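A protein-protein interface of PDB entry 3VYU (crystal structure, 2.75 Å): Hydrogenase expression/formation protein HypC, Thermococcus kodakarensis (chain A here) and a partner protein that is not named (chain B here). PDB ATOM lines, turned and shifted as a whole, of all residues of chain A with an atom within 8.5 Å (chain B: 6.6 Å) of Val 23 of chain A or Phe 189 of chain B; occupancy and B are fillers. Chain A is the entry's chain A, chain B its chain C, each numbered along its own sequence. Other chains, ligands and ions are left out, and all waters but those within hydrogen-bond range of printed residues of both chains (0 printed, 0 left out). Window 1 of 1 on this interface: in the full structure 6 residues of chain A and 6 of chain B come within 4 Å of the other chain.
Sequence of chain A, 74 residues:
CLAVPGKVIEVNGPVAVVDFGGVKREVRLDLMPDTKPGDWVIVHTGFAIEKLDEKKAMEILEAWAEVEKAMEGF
The backbone carbonyl oxygen (O) of Ser 182 of chain B is in hydrogen-bond range of the backbone NH (N) of Ile 187 of chain B. The side-chain carboxylate of Asp 19 of chain A lies within hydrogen-bond range of the backbone NH of Gly 22 of chain A (2.6 Å). The side-chain carboxylate of Asp 19 of chain A is in salt-bridge range of the side-chain amino group of Lys 7 of chain A, at 3.2 Å. The backbone NH (N) of Gly 21 of chain A sits at hydrogen-bond distance from the side-chain carboxylate (OD2) of Asp 19 of chain A (3.4 Å). OD2 of Asp 19 of chain A sits at hydrogen-bond distance from N of Val 23 of chain A (3.2 Å).
Asp 19 of chain A touches Glu 190 of chain B (OD1 to OE1, 3.6 Å). Phe 20 of chain A touches Ala 257 of chain B. CE1 of Phe 189 of chain B touches O of Gly 21 of chain A, 3.6 Å away. Gly 22 of chain A touches Ala 188 of chain B (O to O, 3.9 Å). Gly 22 of chain A touches Phe 189 of chain B. Gly 22 of chain A touches Glu 190 of chain B. Ile 187 of chain B touches Val 23 of chain A. Val 23 of chain A touches Phe 189 of chain B. Met 261 of chain B touches Val 23 of chain A (SD to CB, 3.8 Å). Ala 188 of chain B touches Lys 24 of chain A.
Of the printed residues of chain B, Val 23 of chain A touches Ile 187, Ala 188, Phe 189 and Met 261. Of chain A, only Gly 21, Gly 22 and Val 23 come within 4 Å of Phe 189 of chain B. Of the printed residues of chain A, Ala 188 of chain B touches Gly 22 (3.9 Å), Val 23 (3.9 Å) and Lys 24 (3.7 Å). Of the printed residues of chain A, Met 261 of chain B touches Val 23 (3.8 Å). Of the printed residues of chain B, Gly 22 of chain A touches Ala 188, Phe 189 and Glu 190. Printed residues of chain B within 4 Å of Lys 24 of chain A: Ala 188. Thr 191 of chain B touches none of the printed residues of chain A.
Hydrophobic or aromatic side chains of chain A within 4 Å of the printed part of chain B: Val 23. Along chain A the printed residues that touch a printed residue of chain B span positions 19 to 24. Among the printed residues, 11 pairs touch across the chains.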
ATOM      1  N   VAL A   4     -23.890  28.968  14.188  1.00  0.00           N
ATOM      2  CA  VAL A   4     -23.448  29.159  12.813  1.00  0.00           C
ATOM      3  C   VAL A   4     -23.568  27.789  12.135  1.00  0.00           C
ATOM      4  O   VAL A   4     -23.425  26.755  12.788  1.00  0.00           O
ATOM      5  CB  VAL A   4     -21.979  29.662  12.767  1.00  0.00           C
ATOM      6  CG1 VAL A   4     -21.167  28.998  13.868  1.00  0.00           C
ATOM      7  CG2 VAL A   4     -21.361  29.367  11.408  1.00  0.00           C
ATOM      8  N   PRO A   5     -23.853  27.764  10.824  1.00  0.00           N
ATOM      9  CA  PRO A   5     -23.995  26.502  10.082  1.00  0.00           C
ATOM     10  C   PRO A   5     -22.686  25.840   9.659  1.00  0.00           C
ATOM     11  O   PRO A   5     -21.738  26.514   9.254  1.00  0.00           O
ATOM     12  CB  PRO A   5     -24.840  26.902   8.873  1.00  0.00           C
ATOM     13  CG  PRO A   5     -25.515  28.187   9.309  1.00  0.00           C
ATOM     14  CD  PRO A   5     -24.417  28.878  10.049  1.00  0.00           C
ATOM     15  N   GLY A   6     -22.652  24.510   9.735  1.00  0.00           N
ATOM     16  CA  GLY A   6     -21.454  23.778   9.361  1.00  0.00           C
ATOM     17  C   GLY A   6     -21.678  22.442   8.671  1.00  0.00           C
ATOM     18  O   GLY A   6     -22.632  21.719   8.973  1.00  0.00           O
ATOM     19  N   LYS A   7     -20.776  22.113   7.747  1.00  0.00           N
ATOM     20  CA  LYS A   7     -20.834  20.867   6.985  1.00  0.00           C
ATOM     21  C   LYS A   7     -20.116  19.742   7.719  1.00  0.00           C
ATOM     22  O   LYS A   7     -18.923  19.845   8.012  1.00  0.00           O
ATOM     23  CB  LYS A   7     -20.185  21.054   5.607  1.00  0.00           C
ATOM     24  CG  LYS A   7     -20.298  19.835   4.688  1.00  0.00           C
ATOM     25  CD  LYS A   7     -19.675  20.066   3.307  1.00  0.00           C
ATOM     26  CE  LYS A   7     -18.149  20.031   3.338  1.00  0.00           C
ATOM     27  NZ  LYS A   7     -17.559  21.103   4.185  1.00  0.00           N
ATOM     28  N   ILE A   9     -18.080  16.625   8.111  1.00  0.00           N
ATOM     29  CA  ILE A   9     -17.111  15.967   7.243  1.00  0.00           C
ATOM     30  C   ILE A   9     -16.704  14.595   7.775  1.00  0.00           C
ATOM     31  O   ILE A   9     -16.143  13.780   7.045  1.00  0.00           O
ATOM     32  CB  ILE A   9     -15.851  16.849   7.056  1.00  0.00           C
ATOM     33  CG1 ILE A   9     -15.264  17.229   8.417  1.00  0.00           C
ATOM     34  CG2 ILE A   9     -16.209  18.104   6.270  1.00  0.00           C
ATOM     35  CD1 ILE A   9     -14.024  18.099   8.328  1.00  0.00           C
ATOM     36  N   VAL A  17     -17.902  15.355  13.564  1.00  0.00           N
ATOM     37  CA  VAL A  17     -16.938  16.432  13.353  1.00  0.00           C
ATOM     38  C   VAL A  17     -17.520  17.315  12.263  1.00  0.00           C
ATOM     39  O   VAL A  17     -18.066  16.811  11.284  1.00  0.00           O
ATOM     40  CB  VAL A  17     -15.574  15.895  12.880  1.00  0.00           C
ATOM     41  CG1 VAL A  17     -14.690  17.051  12.402  1.00  0.00           C
ATOM     42  CG2 VAL A  17     -14.901  15.142  14.014  1.00  0.00           C
ATOM     43  N   VAL A  18     -17.403  18.629  12.418  1.00  0.00           N
ATOM     44  CA  VAL A  18     -17.969  19.530  11.426  1.00  0.00           C
ATOM     45  C   VAL A  18     -17.056  20.672  10.984  1.00  0.00           C
ATOM     46  O   VAL A  18     -16.143  21.080  11.705  1.00  0.00           O
ATOM     47  CB  VAL A  18     -19.302  20.113  11.943  1.00  0.00           C
ATOM     48  CG1 VAL A  18     -19.976  20.927  10.857  1.00  0.00           C
ATOM     49  CG2 VAL A  18     -20.214  18.982  12.401  1.00  0.00           C
ATOM     50  N   ASP A  19     -17.327  21.175   9.782  1.00  0.00           N
ATOM     51  CA  ASP A  19     -16.573  22.265   9.166  1.00  0.00           C
ATOM     52  C   ASP A  19     -17.436  23.519   8.981  1.00  0.00           C
ATOM     53  O   ASP A  19     -18.534  23.442   8.429  1.00  0.00           O
ATOM     54  CB  ASP A  19     -16.045  21.805   7.803  1.00  0.00           C
ATOM     55  CG  ASP A  19     -15.542  22.955   6.945  1.00  0.00           C
ATOM     56  OD1 ASP A  19     -15.288  22.725   5.742  1.00  0.00           O
ATOM     57  OD2 ASP A  19     -15.393  24.082   7.462  1.00  0.00           O
ATOM     58  N   PHE A  20     -16.930  24.669   9.427  1.00  0.00           N
ATOM     59  CA  PHE A  20     -17.655  25.936   9.300  1.00  0.00           C
ATOM     60  C   PHE A  20     -16.873  26.939   8.456  1.00  0.00           C
ATOM     61  O   PHE A  20     -16.014  27.650   8.971  1.00  0.00           O
ATOM     62  CB  PHE A  20     -17.920  26.550  10.680  1.00  0.00           C
ATOM     63  CG  PHE A  20     -18.704  25.663  11.604  1.00  0.00           C
ATOM     64  CD1 PHE A  20     -18.066  24.692  12.371  1.00  0.00           C
ATOM     65  CD2 PHE A  20     -20.085  25.786  11.696  1.00  0.00           C
ATOM     66  CE1 PHE A  20     -18.794  23.860  13.220  1.00  0.00           C
ATOM     67  CE2 PHE A  20     -20.821  24.959  12.541  1.00  0.00           C
ATOM     68  CZ  PHE A  20     -20.173  23.993  13.303  1.00  0.00           C
ATOM     69  N   GLY A  21     -17.173  27.002   7.163  1.00  0.00           N
ATOM     70  CA  GLY A  21     -16.465  27.928   6.297  1.00  0.00           C
ATOM     71  C   GLY A  21     -14.973  27.652   6.310  1.00  0.00           C
ATOM     72  O   GLY A  21     -14.177  28.450   5.807  1.00  0.00           O
ATOM     73  N   GLY A  22     -14.595  26.522   6.904  1.00  0.00           N
ATOM     74  CA  GLY A  22     -13.194  26.143   6.962  1.00  0.00           C
ATOM     75  C   GLY A  22     -12.622  25.767   8.318  1.00  0.00           C
ATOM     76  O   GLY A  22     -11.427  25.500   8.427  1.00  0.00           O
ATOM     77  N   VAL A  23     -13.444  25.728   9.358  1.00  0.00           N
ATOM     78  CA  VAL A  23     -12.917  25.384  10.668  1.00  0.00           C
ATOM     79  C   VAL A  23     -13.295  23.973  11.083  1.00  0.00           C
ATOM     80  O   VAL A  23     -14.437  23.550  10.928  1.00  0.00           O
ATOM     81  CB  VAL A  23     -13.405  26.383  11.727  1.00  0.00           C
ATOM     82  CG1 VAL A  23     -12.717  26.113  13.055  1.00  0.00           C
ATOM     83  CG2 VAL A  23     -13.128  27.803  11.253  1.00  0.00           C
ATOM     84  N   LYS A  24     -12.321  23.233  11.596  1.00  0.00           N
ATOM     85  CA  LYS A  24     -12.596  21.879  12.032  1.00  0.00           C
ATOM     86  C   LYS A  24     -12.890  21.918  13.521  1.00  0.00           C
ATOM     87  O   LYS A  24     -12.052  22.329  14.325  1.00  0.00           O
ATOM     88  CB  LYS A  24     -11.411  20.966  11.737  1.00  0.00           C
ATOM     89  N   ARG A  25     -14.102  21.516  13.876  1.00  0.00           N
ATOM     90  CA  ARG A  25     -14.508  21.491  15.267  1.00  0.00           C
ATOM     91  C   ARG A  25     -15.415  20.299  15.502  1.00  0.00           C
ATOM     92  O   ARG A  25     -16.246  19.956  14.660  1.00  0.00           O
ATOM     93  CB  ARG A  25     -15.222  22.781  15.630  1.00  0.00           C
ATOM     94  N   GLU A  26     -15.237  19.667  16.656  1.00  0.00           N
ATOM     95  CA  GLU A  26     -16.024  18.504  17.034  1.00  0.00           C
ATOM     96  C   GLU A  26     -17.421  18.911  17.491  1.00  0.00           C
ATOM     97  O   GLU A  26     -17.619  20.019  17.987  1.00  0.00           O
ATOM     98  CB  GLU A  26     -15.302  17.736  18.143  1.00  0.00           C
ATOM     99  CG  GLU A  26     -13.970  17.146  17.698  1.00  0.00           C
ATOM    100  CD  GLU A  26     -13.222  16.452  18.819  1.00  0.00           C
ATOM    101  OE1 GLU A  26     -13.759  15.477  19.388  1.00  0.00           O
ATOM    102  OE2 GLU A  26     -12.092  16.883  19.128  1.00  0.00           O
ATOM    103  N   VAL A  27     -18.387  18.014  17.324  1.00  0.00           N
ATOM    104  CA  VAL A  27     -19.766  18.296  17.709  1.00  0.00           C
ATOM    105  C   VAL A  27     -20.533  17.057  18.177  1.00  0.00           C
ATOM    106  O   VAL A  27     -20.740  16.115  17.410  1.00  0.00           O
ATOM    107  CB  VAL A  27     -20.549  18.929  16.531  1.00  0.00           C
ATOM    108  CG1 VAL A  27     -22.005  19.141  16.921  1.00  0.00           C
ATOM    109  CG2 VAL A  27     -19.910  20.246  16.127  1.00  0.00           C
ATOM    110  N   SER B 182      -6.978  32.235  16.852  1.00  0.00           N
ATOM    111  CA  SER B 182      -7.307  30.879  16.426  1.00  0.00           C
ATOM    112  C   SER B 182      -6.262  29.886  16.947  1.00  0.00           C
ATOM    113  O   SER B 182      -6.603  28.756  17.299  1.00  0.00           O
ATOM    114  CB  SER B 182      -7.379  30.792  14.890  1.00  0.00           C
ATOM    115  OG  SER B 182      -8.429  31.585  14.357  1.00  0.00           O
ATOM    116  N   GLY B 186      -7.273  26.485  19.652  1.00  0.00           N
ATOM    117  CA  GLY B 186      -7.229  25.195  18.975  1.00  0.00           C
ATOM    118  C   GLY B 186      -7.674  25.231  17.524  1.00  0.00           C
ATOM    119  O   GLY B 186      -7.191  24.451  16.701  1.00  0.00           O
ATOM    120  N   ILE B 187      -8.601  26.135  17.215  1.00  0.00           N
ATOM    121  CA  ILE B 187      -9.127  26.285  15.861  1.00  0.00           C
ATOM    122  C   ILE B 187      -8.031  26.183  14.805  1.00  0.00           C
ATOM    123  O   ILE B 187      -7.134  27.025  14.743  1.00  0.00           O
ATOM    124  CB  ILE B 187      -9.854  27.647  15.691  1.00  0.00           C
ATOM    125  CG1 ILE B 187     -11.205  27.608  16.407  1.00  0.00           C
ATOM    126  CG2 ILE B 187     -10.039  27.971  14.213  1.00  0.00           C
ATOM    127  CD1 ILE B 187     -11.996  28.890  16.284  1.00  0.00           C
ATOM    128  N   ALA B 188      -8.110  25.140  13.985  1.00  0.00           N
ATOM    129  CA  ALA B 188      -7.148  24.916  12.913  1.00  0.00           C
ATOM    130  C   ALA B 188      -7.891  25.141  11.599  1.00  0.00           C
ATOM    131  O   ALA B 188      -9.120  25.051  11.562  1.00  0.00           O
ATOM    132  CB  ALA B 188      -6.610  23.500  12.988  1.00  0.00           C
ATOM    133  N   PHE B 189      -7.152  25.444  10.533  1.00  0.00           N
ATOM    134  CA  PHE B 189      -7.761  25.708   9.232  1.00  0.00           C
ATOM    135  C   PHE B 189      -7.200  24.853   8.097  1.00  0.00           C
ATOM    136  O   PHE B 189      -6.025  24.468   8.100  1.00  0.00           O
ATOM    137  CB  PHE B 189      -7.634  27.199   8.892  1.00  0.00           C
ATOM    138  CG  PHE B 189      -8.951  27.866   8.621  1.00  0.00           C
ATOM    139  CD1 PHE B 189      -9.598  27.697   7.397  1.00  0.00           C
ATOM    140  CD2 PHE B 189      -9.569  28.620   9.609  1.00  0.00           C
ATOM    141  CE1 PHE B 189     -10.845  28.269   7.169  1.00  0.00           C
ATOM    142  CE2 PHE B 189     -10.814  29.195   9.393  1.00  0.00           C
ATOM    143  CZ  PHE B 189     -11.456  29.018   8.170  1.00  0.00           C
ATOM    144  N   GLU B 190      -8.072  24.564   7.132  1.00  0.00           N
ATOM    145  CA  GLU B 190      -7.747  23.749   5.961  1.00  0.00           C
ATOM    146  C   GLU B 190      -6.340  24.134   5.515  1.00  0.00           C
ATOM    147  O   GLU B 190      -5.381  23.384   5.708  1.00  0.00           O
ATOM    148  CB  GLU B 190      -8.770  24.019   4.848  1.00  0.00           C
ATOM    149  CG  GLU B 190     -10.231  24.003   5.321  1.00  0.00           C
ATOM    150  CD  GLU B 190     -11.232  24.253   4.196  1.00  0.00           C
ATOM    151  OE1 GLU B 190     -12.431  24.435   4.492  1.00  0.00           O
ATOM    152  OE2 GLU B 190     -10.835  24.265   3.010  1.00  0.00           O
ATOM    153  N   THR B 191      -6.234  25.312   4.910  1.00  0.00           N
ATOM    154  CA  THR B 191      -4.947  25.860   4.514  1.00  0.00           C
ATOM    155  C   THR B 191      -4.660  26.795   5.673  1.00  0.00           C
ATOM    156  O   THR B 191      -5.499  27.613   6.042  1.00  0.00           O
ATOM    157  CB  THR B 191      -5.034  26.659   3.213  1.00  0.00           C
ATOM    158  OG1 THR B 191      -5.650  25.857   2.199  1.00  0.00           O
ATOM    159  CG2 THR B 191      -3.649  27.057   2.750  1.00  0.00           C
ATOM    160  N   GLU B 192      -3.485  26.662   6.268  1.00  0.00           N
ATOM    161  CA  GLU B 192      -3.180  27.460   7.449  1.00  0.00           C
ATOM    162  C   GLU B 192      -3.448  28.956   7.304  1.00  0.00           C
ATOM    163  O   GLU B 192      -3.064  29.556   6.305  1.00  0.00           O
ATOM    164  CB  GLU B 192      -1.725  27.266   7.881  1.00  0.00           C
ATOM    165  CG  GLU B 192      -1.404  28.058   9.148  1.00  0.00           C
ATOM    166  CD  GLU B 192      -0.006  27.820   9.666  1.00  0.00           C
ATOM    167  OE1 GLU B 192       0.956  28.292   9.024  1.00  0.00           O
ATOM    168  OE2 GLU B 192       0.128  27.155  10.716  1.00  0.00           O
ATOM    169  N   LEU B 193      -4.109  29.551   8.298  1.00  0.00           N
ATOM    170  CA  LEU B 193      -4.376  30.994   8.297  1.00  0.00           C
ATOM    171  C   LEU B 193      -3.259  31.619   9.110  1.00  0.00           C
ATOM    172  O   LEU B 193      -3.081  31.283  10.278  1.00  0.00           O
ATOM    173  CB  LEU B 193      -5.708  31.334   8.971  1.00  0.00           C
ATOM    174  CG  LEU B 193      -5.813  32.802   9.428  1.00  0.00           C
ATOM    175  CD1 LEU B 193      -5.670  33.720   8.230  1.00  0.00           C
ATOM    176  CD2 LEU B 193      -7.134  33.064  10.122  1.00  0.00           C
ATOM    177  N   PRO B 253     -12.079  34.447   3.777  1.00  0.00           N
ATOM    178  CA  PRO B 253     -13.146  33.519   4.138  1.00  0.00           C
ATOM    179  C   PRO B 253     -12.837  32.834   5.468  1.00  0.00           C
ATOM    180  O   PRO B 253     -13.744  32.488   6.224  1.00  0.00           O
ATOM    181  CB  PRO B 253     -13.181  32.565   2.945  1.00  0.00           C
ATOM    182  CG  PRO B 253     -12.723  33.455   1.794  1.00  0.00           C
ATOM    183  CD  PRO B 253     -11.567  34.175   2.422  1.00  0.00           C
ATOM    184  N   GLU B 254     -11.548  32.657   5.751  1.00  0.00           N
ATOM    185  CA  GLU B 254     -11.108  32.030   6.995  1.00  0.00           C
ATOM    186  C   GLU B 254     -11.383  32.998   8.149  1.00  0.00           C
ATOM    187  O   GLU B 254     -11.872  32.602   9.209  1.00  0.00           O
ATOM    188  CB  GLU B 254      -9.600  31.717   6.969  1.00  0.00           C
ATOM    189  CG  GLU B 254      -9.076  30.857   5.809  1.00  0.00           C
ATOM    190  CD  GLU B 254      -8.944  31.630   4.509  1.00  0.00           C
ATOM    191  OE1 GLU B 254      -7.887  31.534   3.849  1.00  0.00           O
ATOM    192  OE2 GLU B 254      -9.903  32.334   4.141  1.00  0.00           O
ATOM    193  N   VAL B 255     -11.057  34.270   7.931  1.00  0.00           N
ATOM    194  CA  VAL B 255     -11.252  35.314   8.935  1.00  0.00           C
ATOM    195  C   VAL B 255     -12.746  35.483   9.264  1.00  0.00           C
ATOM    196  O   VAL B 255     -13.124  35.595  10.434  1.00  0.00           O
ATOM    197  CB  VAL B 255     -10.633  36.667   8.440  1.00  0.00           C
ATOM    198  CG1 VAL B 255     -10.948  37.787   9.407  1.00  0.00           C
ATOM    199  CG2 VAL B 255      -9.118  36.533   8.312  1.00  0.00           C
ATOM    200  N   ALA B 257     -15.228  33.307   9.042  1.00  0.00           N
ATOM    201  CA  ALA B 257     -15.691  32.161   9.803  1.00  0.00           C
ATOM    202  C   ALA B 257     -15.153  32.235  11.226  1.00  0.00           C
ATOM    203  O   ALA B 257     -15.916  32.180  12.186  1.00  0.00           O
ATOM    204  CB  ALA B 257     -15.236  30.863   9.118  1.00  0.00           C
ATOM    205  N   ALA B 258     -13.838  32.384  11.356  1.00  0.00           N
ATOM    206  CA  ALA B 258     -13.208  32.456  12.667  1.00  0.00           C
ATOM    207  C   ALA B 258     -13.772  33.626  13.486  1.00  0.00           C
ATOM    208  O   ALA B 258     -14.047  33.484  14.685  1.00  0.00           O
ATOM    209  CB  ALA B 258     -11.687  32.578  12.509  1.00  0.00           C
ATOM    210  N   MET B 261     -17.198  32.725  14.934  1.00  0.00           N
ATOM    211  CA  MET B 261     -17.065  31.702  15.965  1.00  0.00           C
ATOM    212  C   MET B 261     -16.581  32.287  17.287  1.00  0.00           C
ATOM    213  O   MET B 261     -17.160  32.026  18.344  1.00  0.00           O
ATOM    214  CB  MET B 261     -16.098  30.612  15.501  1.00  0.00           C
ATOM    215  CG  MET B 261     -16.648  29.761  14.375  1.00  0.00           C
ATOM    216  SD  MET B 261     -15.698  28.261  14.128  1.00  0.00           S
ATOM    217  CE  MET B 261     -16.364  27.231  15.418  1.00  0.00           C
